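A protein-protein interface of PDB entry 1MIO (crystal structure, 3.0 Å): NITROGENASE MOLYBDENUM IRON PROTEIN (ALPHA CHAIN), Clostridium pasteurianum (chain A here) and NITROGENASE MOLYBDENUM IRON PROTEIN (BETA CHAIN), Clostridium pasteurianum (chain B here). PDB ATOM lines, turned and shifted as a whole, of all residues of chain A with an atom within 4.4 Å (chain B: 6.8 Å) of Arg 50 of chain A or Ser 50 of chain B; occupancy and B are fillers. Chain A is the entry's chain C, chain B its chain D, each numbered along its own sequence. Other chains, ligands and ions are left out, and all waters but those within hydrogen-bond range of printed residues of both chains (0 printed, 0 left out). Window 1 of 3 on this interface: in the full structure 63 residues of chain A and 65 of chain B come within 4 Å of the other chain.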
ATOM      1  N   ASN A  39       7.264  -9.419  29.227  1.00  0.00           N
ATOM      2  CA  ASN A  39       5.902  -9.352  28.646  1.00  0.00           C
ATOM      3  C   ASN A  39       4.680  -8.484  29.128  1.00  0.00           C
ATOM      4  O   ASN A  39       3.513  -8.881  29.325  1.00  0.00           O
ATOM      5  CB  ASN A  39       5.473 -10.815  28.519  1.00  0.00           C
ATOM      6  CG  ASN A  39       4.424 -11.118  27.458  1.00  0.00           C
ATOM      7  OD1 ASN A  39       3.587 -11.987  27.714  1.00  0.00           O
ATOM      8  ND2 ASN A  39       4.464 -10.577  26.225  1.00  0.00           N
ATOM      9  N   THR A  40       5.052  -7.196  29.118  1.00  0.00           N
ATOM     10  CA  THR A  40       4.220  -6.030  29.408  1.00  0.00           C
ATOM     11  C   THR A  40       4.358  -4.995  28.256  1.00  0.00           C
ATOM     12  O   THR A  40       5.105  -5.216  27.289  1.00  0.00           O
ATOM     13  CB  THR A  40       4.651  -5.316  30.731  1.00  0.00           C
ATOM     14  OG1 THR A  40       5.718  -6.034  31.371  1.00  0.00           O
ATOM     15  CG2 THR A  40       3.397  -5.118  31.591  1.00  0.00           C
ATOM     16  N   THR A  42       5.555  -2.022  25.893  1.00  0.00           N
ATOM     17  CA  THR A  42       6.827  -1.375  25.592  1.00  0.00           C
ATOM     18  C   THR A  42       6.560   0.059  26.069  1.00  0.00           C
ATOM     19  O   THR A  42       5.416   0.559  25.964  1.00  0.00           O
ATOM     20  CB  THR A  42       7.108  -1.376  24.078  1.00  0.00           C
ATOM     21  OG1 THR A  42       7.062  -2.721  23.625  1.00  0.00           O
ATOM     22  CG2 THR A  42       8.419  -0.683  23.762  1.00  0.00           C
ATOM     23  N   THR A  48      12.909   0.383  21.098  1.00  0.00           N
ATOM     24  CA  THR A  48      12.977  -1.069  21.330  1.00  0.00           C
ATOM     25  C   THR A  48      13.187  -1.766  19.979  1.00  0.00           C
ATOM     26  O   THR A  48      13.119  -1.112  18.933  1.00  0.00           O
ATOM     27  CB  THR A  48      11.665  -1.623  21.996  1.00  0.00           C
ATOM     28  OG1 THR A  48      11.922  -2.979  22.458  1.00  0.00           O
ATOM     29  CG2 THR A  48      10.468  -1.451  21.026  1.00  0.00           C
ATOM     30  N   ALA A  49      13.419  -3.093  20.051  1.00  0.00           N
ATOM     31  CA  ALA A  49      13.609  -4.020  18.942  1.00  0.00           C
ATOM     32  C   ALA A  49      12.351  -4.725  18.389  1.00  0.00           C
ATOM     33  O   ALA A  49      12.300  -5.185  17.237  1.00  0.00           O
ATOM     34  CB  ALA A  49      14.604  -5.074  19.397  1.00  0.00           C
ATOM     35  N   ARG A  50      11.340  -4.747  19.259  1.00  0.00           N
ATOM     36  CA  ARG A  50      10.042  -5.420  19.198  1.00  0.00           C
ATOM     37  C   ARG A  50       9.071  -5.103  18.042  1.00  0.00           C
ATOM     38  O   ARG A  50       9.186  -4.057  17.400  1.00  0.00           O
ATOM     39  CB  ARG A  50       9.558  -5.118  20.618  1.00  0.00           C
ATOM     40  CG  ARG A  50       8.352  -5.522  21.420  1.00  0.00           C
ATOM     41  CD  ARG A  50       8.899  -5.478  22.853  1.00  0.00           C
ATOM     42  NE  ARG A  50       7.940  -5.580  23.939  1.00  0.00           N
ATOM     43  CZ  ARG A  50       7.994  -6.494  24.913  1.00  0.00           C
ATOM     44  NH1 ARG A  50       8.914  -7.439  24.972  1.00  0.00           N
ATOM     45  NH2 ARG A  50       7.173  -6.375  25.952  1.00  0.00           N
ATOM     46  N   GLY A  51       8.121  -6.018  17.771  1.00  0.00           N
ATOM     47  CA  GLY A  51       7.124  -5.912  16.713  1.00  0.00           C
ATOM     48  C   GLY A  51       5.644  -5.879  17.146  1.00  0.00           C
ATOM     49  O   GLY A  51       5.266  -5.480  18.249  1.00  0.00           O
ATOM     50  N   VAL A 179       1.571  -7.079  23.333  1.00  0.00           N
ATOM     51  CA  VAL A 179       2.668  -6.138  23.504  1.00  0.00           C
ATOM     52  C   VAL A 179       3.828  -6.367  22.545  1.00  0.00           C
ATOM     53  O   VAL A 179       4.726  -5.543  22.482  1.00  0.00           O
ATOM     54  CB  VAL A 179       3.205  -6.215  24.926  1.00  0.00           C
ATOM     55  CG1 VAL A 179       2.137  -5.666  25.839  1.00  0.00           C
ATOM     56  CG2 VAL A 179       3.624  -7.648  25.297  1.00  0.00           C
ATOM     57  N   SER A 180       3.833  -7.445  21.760  1.00  0.00           N
ATOM     58  CA  SER A 180       4.927  -7.857  20.887  1.00  0.00           C
ATOM     59  C   SER A 180       4.399  -9.003  20.060  1.00  0.00           C
ATOM     60  O   SER A 180       3.313  -9.524  20.339  1.00  0.00           O
ATOM     61  CB  SER A 180       6.122  -8.411  21.647  1.00  0.00           C
ATOM     62  OG  SER A 180       5.883  -9.667  22.287  1.00  0.00           O
ATOM     63  N   GLN A 181       5.221  -9.484  19.130  1.00  0.00           N
ATOM     64  CA  GLN A 181       4.909 -10.656  18.349  1.00  0.00           C
ATOM     65  C   GLN A 181       4.737 -11.973  19.109  1.00  0.00           C
ATOM     66  O   GLN A 181       4.288 -12.937  18.492  1.00  0.00           O
ATOM     67  CB  GLN A 181       5.971 -10.830  17.255  1.00  0.00           C
ATOM     68  CG  GLN A 181       7.431 -11.018  17.577  1.00  0.00           C
ATOM     69  CD  GLN A 181       8.225  -9.741  17.530  1.00  0.00           C
ATOM     70  OE1 GLN A 181       7.724  -8.714  17.921  1.00  0.00           O
ATOM     71  NE2 GLN A 181       9.466  -9.660  17.107  1.00  0.00           N
ATOM     72  N   GLU A 367      13.567  -9.817  23.434  1.00  0.00           N
ATOM     73  CA  GLU A 367      12.806  -8.638  23.088  1.00  0.00           C
ATOM     74  C   GLU A 367      11.374  -9.007  23.151  1.00  0.00           C
ATOM     75  O   GLU A 367      10.633  -8.062  22.984  1.00  0.00           O
ATOM     76  CB  GLU A 367      13.103  -8.095  21.650  1.00  0.00           C
ATOM     77  CG  GLU A 367      12.761  -8.959  20.393  1.00  0.00           C
ATOM     78  CD  GLU A 367      13.471  -8.598  19.085  1.00  0.00           C
ATOM     79  OE1 GLU A 367      14.698  -8.454  19.114  1.00  0.00           O
ATOM     80  OE2 GLU A 367      12.815  -8.491  18.038  1.00  0.00           O
ATOM     81  N   PHE A 368      10.907 -10.251  23.319  1.00  0.00           N
ATOM     82  CA  PHE A 368       9.461 -10.460  23.447  1.00  0.00           C
ATOM     83  C   PHE A 368       8.983 -11.639  24.294  1.00  0.00           C
ATOM     84  O   PHE A 368       7.778 -11.862  24.438  1.00  0.00           O
ATOM     85  CB  PHE A 368       8.840 -10.549  22.020  1.00  0.00           C
ATOM     86  CG  PHE A 368       9.129 -11.807  21.230  1.00  0.00           C
ATOM     87  CD1 PHE A 368       8.410 -12.957  21.472  1.00  0.00           C
ATOM     88  CD2 PHE A 368      10.127 -11.811  20.307  1.00  0.00           C
ATOM     89  CE1 PHE A 368       8.672 -14.127  20.832  1.00  0.00           C
ATOM     90  CE2 PHE A 368      10.388 -12.982  19.662  1.00  0.00           C
ATOM     91  CZ  PHE A 368       9.667 -14.116  19.926  1.00  0.00           C
ATOM     92  N   ASP A 441      15.202  -7.569  29.570  1.00  0.00           N
ATOM     93  CA  ASP A 441      14.045  -7.796  28.752  1.00  0.00           C
ATOM     94  C   ASP A 441      13.674  -6.427  28.176  1.00  0.00           C
ATOM     95  O   ASP A 441      13.637  -5.417  28.897  1.00  0.00           O
ATOM     96  CB  ASP A 441      12.931  -8.386  29.579  1.00  0.00           C
ATOM     97  CG  ASP A 441      11.711  -8.651  28.702  1.00  0.00           C
ATOM     98  OD1 ASP A 441      11.552  -9.708  28.096  1.00  0.00           O
ATOM     99  OD2 ASP A 441      10.867  -7.764  28.609  1.00  0.00           O
ATOM    100  N   ASP A 442      13.352  -6.521  26.861  1.00  0.00           N
ATOM    101  CA  ASP A 442      13.147  -5.530  25.808  1.00  0.00           C
ATOM    102  C   ASP A 442      14.112  -4.356  25.885  1.00  0.00           C
ATOM    103  O   ASP A 442      13.875  -3.152  25.812  1.00  0.00           O
ATOM    104  CB  ASP A 442      11.614  -5.070  25.697  1.00  0.00           C
ATOM    105  CG  ASP A 442      10.796  -3.993  26.426  1.00  0.00           C
ATOM    106  OD1 ASP A 442      10.924  -2.800  26.150  1.00  0.00           O
ATOM    107  OD2 ASP A 442       9.929  -4.340  27.233  1.00  0.00           O
ATOM    108  N   MET B  29       9.809   8.817   7.153  1.00  0.00           N
ATOM    109  CA  MET B  29      10.989   8.550   7.958  1.00  0.00           C
ATOM    110  C   MET B  29      12.265   8.956   7.231  1.00  0.00           C
ATOM    111  O   MET B  29      13.159   9.477   7.887  1.00  0.00           O
ATOM    112  CB  MET B  29      11.076   7.080   8.294  1.00  0.00           C
ATOM    113  CG  MET B  29      12.291   6.795   9.151  1.00  0.00           C
ATOM    114  SD  MET B  29      12.533   5.076   9.633  1.00  0.00           S
ATOM    115  CE  MET B  29      10.989   4.747  10.449  1.00  0.00           C
ATOM    116  N   SER B  42       7.273   7.253  14.829  1.00  0.00           N
ATOM    117  CA  SER B  42       6.031   6.626  14.342  1.00  0.00           C
ATOM    118  C   SER B  42       4.930   6.665  15.405  1.00  0.00           C
ATOM    119  O   SER B  42       5.074   6.257  16.579  1.00  0.00           O
ATOM    120  CB  SER B  42       6.204   5.158  13.973  1.00  0.00           C
ATOM    121  OG  SER B  42       6.926   4.981  12.744  1.00  0.00           O
ATOM    122  N   SER B  45       1.011   1.598  16.176  1.00  0.00           N
ATOM    123  CA  SER B  45       1.630   0.437  16.779  1.00  0.00           C
ATOM    124  C   SER B  45       3.115   0.358  16.403  1.00  0.00           C
ATOM    125  O   SER B  45       3.707   0.981  15.503  1.00  0.00           O
ATOM    126  CB  SER B  45       0.859  -0.819  16.358  1.00  0.00           C
ATOM    127  OG  SER B  45       1.376  -2.014  16.934  1.00  0.00           O
ATOM    128  N   GLN B  46       3.766  -0.459  17.189  1.00  0.00           N
ATOM    129  CA  GLN B  46       5.200  -0.541  17.089  1.00  0.00           C
ATOM    130  C   GLN B  46       5.721  -1.444  16.005  1.00  0.00           C
ATOM    131  O   GLN B  46       6.916  -1.433  15.709  1.00  0.00           O
ATOM    132  CB  GLN B  46       5.759  -0.961  18.429  1.00  0.00           C
ATOM    133  CG  GLN B  46       4.880  -1.739  19.378  1.00  0.00           C
ATOM    134  CD  GLN B  46       5.790  -2.421  20.359  1.00  0.00           C
ATOM    135  OE1 GLN B  46       6.687  -1.797  20.932  1.00  0.00           O
ATOM    136  NE2 GLN B  46       5.611  -3.722  20.515  1.00  0.00           N
ATOM    137  N   GLY B  47       4.836  -2.197  15.356  1.00  0.00           N
ATOM    138  CA  GLY B  47       5.239  -3.078  14.280  1.00  0.00           C
ATOM    139  C   GLY B  47       5.804  -2.297  13.127  1.00  0.00           C
ATOM    140  O   GLY B  47       6.892  -2.582  12.660  1.00  0.00           O
ATOM    141  N   CYS B  48       5.071  -1.252  12.754  1.00  0.00           N
ATOM    142  CA  CYS B  48       5.415  -0.307  11.702  1.00  0.00           C
ATOM    143  C   CYS B  48       6.729   0.404  11.836  1.00  0.00           C
ATOM    144  O   CYS B  48       7.215   0.955  10.863  1.00  0.00           O
ATOM    145  CB  CYS B  48       4.436   0.774  11.612  1.00  0.00           C
ATOM    146  SG  CYS B  48       2.816   0.102  11.318  1.00  0.00           S
ATOM    147  N   CYS B  49       7.301   0.505  13.016  1.00  0.00           N
ATOM    148  CA  CYS B  49       8.562   1.171  13.192  1.00  0.00           C
ATOM    149  C   CYS B  49       9.657   0.189  12.787  1.00  0.00           C
ATOM    150  O   CYS B  49      10.557   0.555  12.009  1.00  0.00           O
ATOM    151  CB  CYS B  49       8.685   1.561  14.636  1.00  0.00           C
ATOM    152  SG  CYS B  49       9.900   2.857  14.917  1.00  0.00           S
ATOM    153  N   SER B  50       9.498  -1.082  13.221  1.00  0.00           N
ATOM    154  CA  SER B  50      10.524  -2.093  13.070  1.00  0.00           C
ATOM    155  C   SER B  50      10.710  -2.357  11.594  1.00  0.00           C
ATOM    156  O   SER B  50      11.831  -2.233  11.073  1.00  0.00           O
ATOM    157  CB  SER B  50      10.130  -3.374  13.802  1.00  0.00           C
ATOM    158  OG  SER B  50       8.918  -3.933  13.324  1.00  0.00           O
ATOM    159  N   TYR B  51       9.586  -2.630  10.927  1.00  0.00           N
ATOM    160  CA  TYR B  51       9.543  -2.837   9.510  1.00  0.00           C
ATOM    161  C   TYR B  51      10.244  -1.738   8.728  1.00  0.00           C
ATOM    162  O   TYR B  51      11.167  -2.052   7.986  1.00  0.00           O
ATOM    163  CB  TYR B  51       8.092  -2.951   9.108  1.00  0.00           C
ATOM    164  CG  TYR B  51       7.445  -4.314   9.328  1.00  0.00           C
ATOM    165  CD1 TYR B  51       8.218  -5.407   9.677  1.00  0.00           C
ATOM    166  CD2 TYR B  51       6.087  -4.473   9.128  1.00  0.00           C
ATOM    167  CE1 TYR B  51       7.649  -6.647   9.821  1.00  0.00           C
ATOM    168  CE2 TYR B  51       5.521  -5.714   9.266  1.00  0.00           C
ATOM    169  CZ  TYR B  51       6.308  -6.791   9.614  1.00  0.00           C
ATOM    170  OH  TYR B  51       5.779  -8.064   9.721  1.00  0.00           O
ATOM    171  N   HIS B  52       9.961  -0.444   8.927  1.00  0.00           N
ATOM    172  CA  HIS B  52      10.509   0.649   8.124  1.00  0.00           C
ATOM    173  C   HIS B  52      11.975   0.945   8.404  1.00  0.00           C
ATOM    174  O   HIS B  52      12.732   1.227   7.484  1.00  0.00           O
ATOM    175  CB  HIS B  52       9.689   1.903   8.362  1.00  0.00           C
ATOM    176  CG  HIS B  52       8.185   1.740   8.255  1.00  0.00           C
ATOM    177  ND1 HIS B  52       7.254   2.560   8.680  1.00  0.00           N
ATOM    178  CD2 HIS B  52       7.505   0.671   7.738  1.00  0.00           C
ATOM    179  CE1 HIS B  52       6.080   2.020   8.431  1.00  0.00           C
ATOM    180  NE2 HIS B  52       6.233   0.873   7.861  1.00  0.00           N
ATOM    181  N   ARG B  53      12.423   0.899   9.658  1.00  0.00           N
ATOM    182  CA  ARG B  53      13.833   1.065   9.987  1.00  0.00           C
ATOM    183  C   ARG B  53      14.615  -0.125   9.458  1.00  0.00           C
ATOM    184  O   ARG B  53      15.722   0.097   8.963  1.00  0.00           O
ATOM    185  CB  ARG B  53      14.096   1.125  11.473  1.00  0.00           C
ATOM    186  CG  ARG B  53      13.332   2.233  12.146  1.00  0.00           C
ATOM    187  CD  ARG B  53      13.371   2.030  13.648  1.00  0.00           C
ATOM    188  NE  ARG B  53      14.723   2.090  14.164  1.00  0.00           N
ATOM    189  CZ  ARG B  53      15.076   1.327  15.185  1.00  0.00           C
ATOM    190  NH1 ARG B  53      14.205   0.504  15.759  1.00  0.00           N
ATOM    191  NH2 ARG B  53      16.324   1.332  15.601  1.00  0.00           N
ATOM    192  N   THR B  54      14.089  -1.366   9.535  1.00  0.00           N
ATOM    193  CA  THR B  54      14.719  -2.551   8.956  1.00  0.00           C
ATOM    194  C   THR B  54      14.874  -2.423   7.426  1.00  0.00           C
ATOM    195  O   THR B  54      15.945  -2.733   6.942  1.00  0.00           O
ATOM    196  CB  THR B  54      13.854  -3.794   9.370  1.00  0.00           C
ATOM    197  OG1 THR B  54      13.942  -4.051  10.790  1.00  0.00           O
ATOM    198  CG2 THR B  54      14.318  -5.004   8.594  1.00  0.00           C
ATOM    199  N   VAL B  55      13.919  -1.992   6.599  1.00  0.00           N
ATOM    200  CA  VAL B  55      14.121  -1.722   5.178  1.00  0.00           C
ATOM    201  C   VAL B  55      15.135  -0.610   4.953  1.00  0.00           C
ATOM    202  O   VAL B  55      16.014  -0.761   4.109  1.00  0.00           O
ATOM    203  CB  VAL B  55      12.747  -1.374   4.501  1.00  0.00           C
ATOM    204  CG1 VAL B  55      12.323   0.055   4.656  1.00  0.00           C
ATOM    205  CG2 VAL B  55      12.870  -1.679   3.034  1.00  0.00           C
ATOM    206  N   THR B  68       8.623   4.853  18.876  1.00  0.00           N
ATOM    207  CA  THR B  68       7.171   4.736  18.746  1.00  0.00           C
ATOM    208  C   THR B  68       6.308   5.136  19.976  1.00  0.00           C
ATOM    209  O   THR B  68       6.684   5.130  21.165  1.00  0.00           O
ATOM    210  CB  THR B  68       6.697   3.295  18.384  1.00  0.00           C
ATOM    211  OG1 THR B  68       7.767   2.367  18.537  1.00  0.00           O
ATOM    212  CG2 THR B  68       6.073   3.298  17.015  1.00  0.00           C
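Of the 14 printed residues of chain A, 5 touch a printed residue of chain B. Of the 14 printed residues of chain B, 3 touch a printed residue of chain A. Printed residues of chain B that touch a printed residue of chain A: Gln 46, Ser 50 and Arg 53. Among the printed residues, no Asp or Glu carboxylate lies within 4 Å of a Lys or Arg side-chain nitrogen of the other chain.
O of Gly 47 of chain B is in hydrogen-bond range of OG of Ser 50 of chain B, at 2.5 Å. The side-chain amide oxygen (OE1) of Gln 181 of chain A is in hydrogen-bond range of the backbone NH (N) of Gly 51 of chain A (2.7 Å). NH1 of Arg 50 of chain A sits at hydrogen-bond distance from O of Glu 367 of chain A, 2.7 Å away. The backbone carbonyl oxygen (O) of Thr 40 of chain A is in hydrogen-bond range of the guanidinium group (NH2) of Arg 50 of chain A (2.7 Å). The backbone carbonyl oxygen (O) of Ser 50 of chain B sits at hydrogen-bond distance from the side-chain hydroxyl (OG1) of Thr 54 of chain B, at 2.8 Å. The side-chain hydroxyl of Thr 42 of chain A sits at hydrogen-bond distance from the guanidinium group of Arg 50 of chain A, 3.0 Å away.
O of Gly 51 of chain A is in hydrogen-bond range of NE2 of Gln 46 of chain B, 2.9 Å away. O of Val 179 of chain A is in hydrogen-bond range of NE2 of Gln 46 of chain B, at 2.8 Å. OG1 of Thr 42 of chain A is in hydrogen-bond range of OE1 of Gln 46 of chain B, 2.9 Å away.
Printed residues of chain B within 4 Å of Thr 42 of chain A: Gln 46 (2.9 Å). Of the printed residues of chain B, Thr 48 of chain A touches Gln 46 and Arg 53. Ala 49 of chain A touches none of the printed residues of chain B. Of the printed residues of chain B, Arg 50 of chain A touches Gln 46 (3.4 Å) and Ser 50 (3.8 Å). Glu 367 of chain A touches none of the printed residues of chain B. Ser 50 of chain B touches just one residue of chain A: Arg 50 (3.8 Å). The nearest residue of chain A that does not touch Ser 50 of chain B is Gly 51 of chain A (4.3 Å).
CG2 of Thr 48 of chain A touches OE1 of Gln 46 of chain B, at 3.8 Å. O of Thr 48 of chain A touches NH1 of Arg 53 of chain B (3.7 Å). CG of Arg 50 of chain A touches NE2 of Gln 46 of chain B (3.4 Å). Arg 50 of chain A touches Ser 50 of chain B (O to CB, 3.8 Å).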
